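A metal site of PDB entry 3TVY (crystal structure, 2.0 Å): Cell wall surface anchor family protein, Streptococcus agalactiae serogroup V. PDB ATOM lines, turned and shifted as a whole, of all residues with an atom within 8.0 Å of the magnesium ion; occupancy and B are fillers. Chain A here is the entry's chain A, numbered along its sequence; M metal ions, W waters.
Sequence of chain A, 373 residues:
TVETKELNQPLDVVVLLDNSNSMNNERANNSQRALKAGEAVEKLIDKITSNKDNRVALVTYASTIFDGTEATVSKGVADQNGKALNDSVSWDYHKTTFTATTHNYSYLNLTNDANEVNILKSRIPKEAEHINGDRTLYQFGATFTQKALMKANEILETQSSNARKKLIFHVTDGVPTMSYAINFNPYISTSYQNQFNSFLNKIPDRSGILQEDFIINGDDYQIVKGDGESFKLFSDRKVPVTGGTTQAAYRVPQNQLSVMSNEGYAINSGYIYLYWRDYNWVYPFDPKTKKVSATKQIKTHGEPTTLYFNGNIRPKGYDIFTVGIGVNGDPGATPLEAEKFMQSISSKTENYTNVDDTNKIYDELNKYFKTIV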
ATOM      1  N   ASP A  18      20.671 -35.588   7.888  1.00  0.00           N
ATOM      2  CA  ASP A  18      20.568 -34.293   8.575  1.00  0.00           C
ATOM      3  C   ASP A  18      19.443 -33.477   7.895  1.00  0.00           C
ATOM      4  O   ASP A  18      19.439 -33.328   6.695  1.00  0.00           O
ATOM      5  CB  ASP A  18      21.964 -33.650   8.562  1.00  0.00           C
ATOM      6  CG  ASP A  18      22.047 -32.261   9.201  1.00  0.00           C
ATOM      7  OD1 ASP A  18      21.033 -31.563   9.356  1.00  0.00           O
ATOM      8  OD2 ASP A  18      23.201 -31.853   9.487  1.00  0.00           O
ATOM      9  N   ASN A  19      18.463 -33.056   8.675  1.00  0.00           N
ATOM     10  CA  ASN A  19      17.318 -32.229   8.216  1.00  0.00           C
ATOM     11  C   ASN A  19      17.270 -30.912   9.032  1.00  0.00           C
ATOM     12  O   ASN A  19      16.216 -30.317   9.235  1.00  0.00           O
ATOM     13  CB  ASN A  19      16.007 -33.033   8.313  1.00  0.00           C
ATOM     14  CG  ASN A  19      14.835 -32.398   7.559  1.00  0.00           C
ATOM     15  OD1 ASN A  19      14.936 -32.033   6.381  1.00  0.00           O
ATOM     16  ND2 ASN A  19      13.727 -32.246   8.229  1.00  0.00           N
ATOM     17  N   SER A  20      18.431 -30.489   9.535  1.00  0.00           N
ATOM     18  CA  SER A  20      18.549 -29.213  10.221  1.00  0.00           C
ATOM     19  C   SER A  20      18.084 -28.022   9.348  1.00  0.00           C
ATOM     20  O   SER A  20      18.089 -28.110   8.101  1.00  0.00           O
ATOM     21  CB  SER A  20      20.000 -29.011  10.712  1.00  0.00           C
ATOM     22  OG  SER A  20      20.938 -28.933   9.634  1.00  0.00           O
ATOM     23  N   ASN A  21      17.665 -26.922   9.998  1.00  0.00           N
ATOM     24  CA  ASN A  21      17.216 -25.651   9.324  1.00  0.00           C
ATOM     25  C   ASN A  21      18.175 -25.133   8.248  1.00  0.00           C
ATOM     26  O   ASN A  21      17.741 -24.580   7.227  1.00  0.00           O
ATOM     27  CB  ASN A  21      17.000 -24.529  10.363  1.00  0.00           C
ATOM     28  CG  ASN A  21      15.868 -24.844  11.319  1.00  0.00           C
ATOM     29  OD1 ASN A  21      14.987 -25.647  11.007  1.00  0.00           O
ATOM     30  ND2 ASN A  21      15.877 -24.193  12.479  1.00  0.00           N
ATOM     31  N   SER A  22      19.481 -25.328   8.490  1.00  0.00           N
ATOM     32  CA  SER A  22      20.501 -24.940   7.549  1.00  0.00           C
ATOM     33  C   SER A  22      20.413 -25.711   6.197  1.00  0.00           C
ATOM     34  O   SER A  22      20.985 -25.279   5.194  1.00  0.00           O
ATOM     35  CB  SER A  22      21.887 -25.148   8.150  1.00  0.00           C
ATOM     36  OG  SER A  22      22.196 -26.531   8.088  1.00  0.00           O
ATOM     37  N   MET A  23      19.675 -26.835   6.181  1.00  0.00           N
ATOM     38  CA  MET A  23      19.491 -27.646   4.952  1.00  0.00           C
ATOM     39  C   MET A  23      18.388 -27.090   4.018  1.00  0.00           C
ATOM     40  O   MET A  23      18.268 -27.532   2.841  1.00  0.00           O
ATOM     41  CB  MET A  23      19.157 -29.121   5.280  1.00  0.00           C
ATOM     42  CG  MET A  23      20.307 -29.936   5.905  1.00  0.00           C
ATOM     43  SD  MET A  23      21.630 -30.413   4.742  1.00  0.00           S
ATOM     44  CE  MET A  23      20.849 -31.757   3.824  1.00  0.00           C
ATOM     45  N   ASN A  24      17.588 -26.171   4.529  1.00  0.00           N
ATOM     46  CA  ASN A  24      16.447 -25.633   3.774  1.00  0.00           C
ATOM     47  C   ASN A  24      16.919 -25.188   2.387  1.00  0.00           C
ATOM     48  O   ASN A  24      18.005 -24.604   2.248  1.00  0.00           O
ATOM     49  CB  ASN A  24      15.803 -24.485   4.515  1.00  0.00           C
ATOM     50  CG  ASN A  24      14.773 -23.757   3.670  1.00  0.00           C
ATOM     51  OD1 ASN A  24      15.137 -22.880   2.860  1.00  0.00           O
ATOM     52  ND2 ASN A  24      13.493 -24.098   3.842  1.00  0.00           N
ATOM     53  N   ARG A  27      18.747 -21.910   1.437  1.00  0.00           N
ATOM     54  CA  ARG A  27      19.978 -21.531   2.125  1.00  0.00           C
ATOM     55  C   ARG A  27      21.196 -21.879   1.277  1.00  0.00           C
ATOM     56  O   ARG A  27      21.080 -22.627   0.280  1.00  0.00           O
ATOM     57  CB  ARG A  27      20.070 -22.219   3.510  1.00  0.00           C
ATOM     58  CG  ARG A  27      18.987 -21.743   4.467  1.00  0.00           C
ATOM     59  CD  ARG A  27      19.462 -20.699   5.466  1.00  0.00           C
ATOM     60  NE  ARG A  27      18.405 -20.321   6.431  1.00  0.00           N
ATOM     61  CZ  ARG A  27      18.410 -20.625   7.732  1.00  0.00           C
ATOM     62  NH1 ARG A  27      19.406 -21.310   8.269  1.00  0.00           N
ATOM     63  NH2 ARG A  27      17.421 -20.227   8.525  1.00  0.00           N
ATOM     64  N   ARG A  33      20.110 -27.946  -0.586  1.00  0.00           N
ATOM     65  CA  ARG A  33      20.731 -29.019   0.174  1.00  0.00           C
ATOM     66  C   ARG A  33      19.752 -30.179   0.491  1.00  0.00           C
ATOM     67  O   ARG A  33      20.067 -31.327   0.190  1.00  0.00           O
ATOM     68  CB  ARG A  33      21.364 -28.453   1.445  1.00  0.00           C
ATOM     69  CG  ARG A  33      22.516 -27.502   1.212  1.00  0.00           C
ATOM     70  CD  ARG A  33      23.163 -27.163   2.516  1.00  0.00           C
ATOM     71  NE  ARG A  33      24.439 -26.455   2.337  1.00  0.00           N
ATOM     72  CZ  ARG A  33      25.108 -25.879   3.326  1.00  0.00           C
ATOM     73  NH1 ARG A  33      24.634 -25.919   4.557  1.00  0.00           N
ATOM     74  NH2 ARG A  33      26.255 -25.263   3.077  1.00  0.00           N
ATOM     75  N   TYR A  61      17.286 -36.687  11.194  1.00  0.00           N
ATOM     76  CA  TYR A  61      17.529 -36.025  12.455  1.00  0.00           C
ATOM     77  C   TYR A  61      17.801 -34.506  12.353  1.00  0.00           C
ATOM     78  O   TYR A  61      18.284 -34.011  11.316  1.00  0.00           O
ATOM     79  CB  TYR A  61      18.670 -36.736  13.207  1.00  0.00           C
ATOM     80  CG  TYR A  61      20.051 -36.344  12.746  1.00  0.00           C
ATOM     81  CD1 TYR A  61      20.721 -35.269  13.320  1.00  0.00           C
ATOM     82  CD2 TYR A  61      20.676 -37.040  11.712  1.00  0.00           C
ATOM     83  CE1 TYR A  61      22.023 -34.911  12.872  1.00  0.00           C
ATOM     84  CE2 TYR A  61      21.942 -36.687  11.262  1.00  0.00           C
ATOM     85  CZ  TYR A  61      22.614 -35.622  11.835  1.00  0.00           C
ATOM     86  OH  TYR A  61      23.881 -35.297  11.368  1.00  0.00           O
ATOM     87  N   ALA A  62      17.478 -33.791  13.425  1.00  0.00           N
ATOM     88  CA  ALA A  62      17.955 -32.423  13.637  1.00  0.00           C
ATOM     89  C   ALA A  62      18.124 -32.262  15.154  1.00  0.00           C
ATOM     90  O   ALA A  62      19.041 -32.848  15.708  1.00  0.00           O
ATOM     91  CB  ALA A  62      17.001 -31.354  13.006  1.00  0.00           C
ATOM     92  N   GLY A 141      15.092 -27.608  14.538  1.00  0.00           N
ATOM     93  CA  GLY A 141      16.001 -27.689  13.393  1.00  0.00           C
ATOM     94  C   GLY A 141      17.503 -27.576  13.677  1.00  0.00           C
ATOM     95  O   GLY A 141      18.283 -27.237  12.770  1.00  0.00           O
ATOM     96  N   ALA A 142      17.912 -27.834  14.919  1.00  0.00           N
ATOM     97  CA  ALA A 142      19.340 -27.821  15.266  1.00  0.00           C
ATOM     98  C   ALA A 142      20.020 -29.187  14.931  1.00  0.00           C
ATOM     99  O   ALA A 142      19.464 -29.978  14.166  1.00  0.00           O
ATOM    100  CB  ALA A 142      19.539 -27.441  16.704  1.00  0.00           C
ATOM    101  N   THR A 143      21.212 -29.436  15.465  1.00  0.00           N
ATOM    102  CA  THR A 143      22.033 -30.580  15.066  1.00  0.00           C
ATOM    103  C   THR A 143      22.497 -31.434  16.261  1.00  0.00           C
ATOM    104  O   THR A 143      23.540 -31.167  16.895  1.00  0.00           O
ATOM    105  CB  THR A 143      23.222 -30.134  14.191  1.00  0.00           C
ATOM    106  OG1 THR A 143      22.772 -29.237  13.163  1.00  0.00           O
ATOM    107  CG2 THR A 143      23.896 -31.328  13.534  1.00  0.00           C
ATOM    108  N   THR A 172      25.334 -35.053   6.285  1.00  0.00           N
ATOM    109  CA  THR A 172      25.196 -33.928   7.230  1.00  0.00           C
ATOM    110  C   THR A 172      25.789 -32.623   6.684  1.00  0.00           C
ATOM    111  O   THR A 172      26.662 -32.631   5.813  1.00  0.00           O
ATOM    112  CB  THR A 172      25.821 -34.275   8.624  1.00  0.00           C
ATOM    113  OG1 THR A 172      25.621 -33.196   9.541  1.00  0.00           O
ATOM    114  CG2 THR A 172      27.344 -34.537   8.507  1.00  0.00           C
ATOM    115  N   ASP A 173      25.294 -31.494   7.178  1.00  0.00           N
ATOM    116  CA  ASP A 173      25.893 -30.201   6.817  1.00  0.00           C
ATOM    117  C   ASP A 173      26.299 -29.400   8.060  1.00  0.00           C
ATOM    118  O   ASP A 173      26.445 -28.179   7.990  1.00  0.00           O
ATOM    119  CB  ASP A 173      24.961 -29.379   5.912  1.00  0.00           C
ATOM    120  CG  ASP A 173      23.848 -28.642   6.697  1.00  0.00           C
ATOM    121  OD1 ASP A 173      23.606 -28.969   7.899  1.00  0.00           O
ATOM    122  OD2 ASP A 173      23.227 -27.751   6.093  1.00  0.00           O
ATOM    123  N   GLY A 174      26.479 -30.077   9.212  1.00  0.00           N
ATOM    124  CA  GLY A 174      26.878 -29.300  10.395  1.00  0.00           C
ATOM    125  C   GLY A 174      27.460 -30.081  11.539  1.00  0.00           C
ATOM    126  O   GLY A 174      27.058 -31.249  11.779  1.00  0.00           O
ATOM    127  N   VAL A 175      28.414 -29.478  12.237  1.00  0.00           N
ATOM    128  CA  VAL A 175      28.856 -30.012  13.525  1.00  0.00           C
ATOM    129  C   VAL A 175      27.690 -30.005  14.554  1.00  0.00           C
ATOM    130  O   VAL A 175      26.749 -29.219  14.421  1.00  0.00           O
ATOM    131  CB  VAL A 175      30.069 -29.223  14.097  1.00  0.00           C
ATOM    132  CG1 VAL A 175      31.324 -29.452  13.239  1.00  0.00           C
ATOM    133  CG2 VAL A 175      29.752 -27.704  14.283  1.00  0.00           C
ATOM    134  N   THR A 177      25.392 -29.232  17.678  1.00  0.00           N
ATOM    135  CA  THR A 177      25.111 -28.073  18.509  1.00  0.00           C
ATOM    136  C   THR A 177      24.310 -28.488  19.753  1.00  0.00           C
ATOM    137  O   THR A 177      23.761 -27.652  20.489  1.00  0.00           O
ATOM    138  CB  THR A 177      24.371 -26.982  17.708  1.00  0.00           C
ATOM    139  OG1 THR A 177      23.163 -27.518  17.160  1.00  0.00           O
ATOM    140  CG2 THR A 177      25.281 -26.426  16.594  1.00  0.00           C
ATOM    141  N   ILE A 325      28.204 -31.553   3.708  1.00  0.00           N
ATOM    142  CA  ILE A 325      27.791 -30.583   2.709  1.00  0.00           C
ATOM    143  C   ILE A 325      28.200 -29.155   3.086  1.00  0.00           C
ATOM    144  O   ILE A 325      27.521 -28.500   3.902  1.00  0.00           O
ATOM    145  CB  ILE A 325      26.268 -30.626   2.414  1.00  0.00           C
ATOM    146  CG1 ILE A 325      25.758 -32.073   2.308  1.00  0.00           C
ATOM    147  CG2 ILE A 325      25.986 -29.835   1.119  1.00  0.00           C
ATOM    148  CD1 ILE A 325      24.228 -32.213   2.454  1.00  0.00           C
ATOM    149  N   ASP A 330      30.548 -23.829  11.325  1.00  0.00           N
ATOM    150  CA  ASP A 330      29.509 -22.932  11.815  1.00  0.00           C
ATOM    151  C   ASP A 330      28.349 -23.683  12.481  1.00  0.00           C
ATOM    152  O   ASP A 330      27.913 -24.716  12.003  1.00  0.00           O
ATOM    153  CB  ASP A 330      29.036 -21.996  10.694  1.00  0.00           C
ATOM    154  CG  ASP A 330      30.114 -21.004  10.285  1.00  0.00           C
ATOM    155  OD1 ASP A 330      31.077 -20.866  11.045  1.00  0.00           O
ATOM    156  OD2 ASP A 330      30.009 -20.386   9.207  1.00  0.00           O
ATOM    157  N   PRO A 331      27.864 -23.184  13.628  1.00  0.00           N
ATOM    158  CA  PRO A 331      28.338 -22.021  14.408  1.00  0.00           C
ATOM    159  C   PRO A 331      29.282 -22.470  15.528  1.00  0.00           C
ATOM    160  O   PRO A 331      28.986 -23.417  16.246  1.00  0.00           O
ATOM    161  CB  PRO A 331      27.025 -21.439  14.986  1.00  0.00           C
ATOM    162  CG  PRO A 331      26.125 -22.639  15.139  1.00  0.00           C
ATOM    163  CD  PRO A 331      26.588 -23.710  14.143  1.00  0.00           C
HETATM  164 MG    MG M   1      22.844 -27.932   9.470  1.00  0.00          MG
HETATM  165  O   HOH W   1      24.639 -26.976   9.540  1.00  0.00           O
HETATM  166  O   HOH W   2      23.624 -29.512  10.643  1.00  0.00           O
HETATM  167  O   HOH W   3      22.328 -26.775  11.186  1.00  0.00           O
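OD2 of Asp 18 is in hydrogen-bond range of N of Asp 173 (3.1 Å).
NH1 of Arg 33 is in salt-bridge range of OD2 of Asp 173, 2.8 Å away.
The backbone NH (N) of Ser 20 is in hydrogen-bond range of the side-chain carboxylate (OD1) of Asp 18, 2.8 Å away.
The backbone NH (N) of Thr 177 lies within hydrogen-bond range of the backbone carbonyl oxygen (O) of Thr 143, at 2.8 Å.
The side-chain carboxylate (OD2) of Asp 18 is in hydrogen-bond range of the side-chain hydroxyl (OG1) of Thr 172 (2.8 Å).
Residues that only touch the magnesium ion: Thr 143 (3.9 Å) and Asp 18 (3.9 Å).
Five residues have an atom within 4 Å of the magnesium ion: Asp 18, Ser 20, Ser 22, Thr 143 and Asp 173.
The magnesium ion is bound by the side-chain carboxylate (OD1) of Asp 173 (2.0 Å).
The magnesium ion is bound by water W1, at 2.0 Å.
The magnesium ion is bound by OG of Ser 22.
Water W2 is bound to the magnesium ion (2.1 Å).
Water W3 is bound to the magnesium ion, at 2.1 Å.
OG of Ser 20 binds the magnesium ion (2.2 Å).
The magnesium ion has six donor atoms within binding distance.
Water W2 lies within hydrogen-bond range of the side-chain carboxylate (OD2) of Asp 18, the side-chain hydroxyl (OG1) of Thr 143 and the backbone NH (N) of Gly 174.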
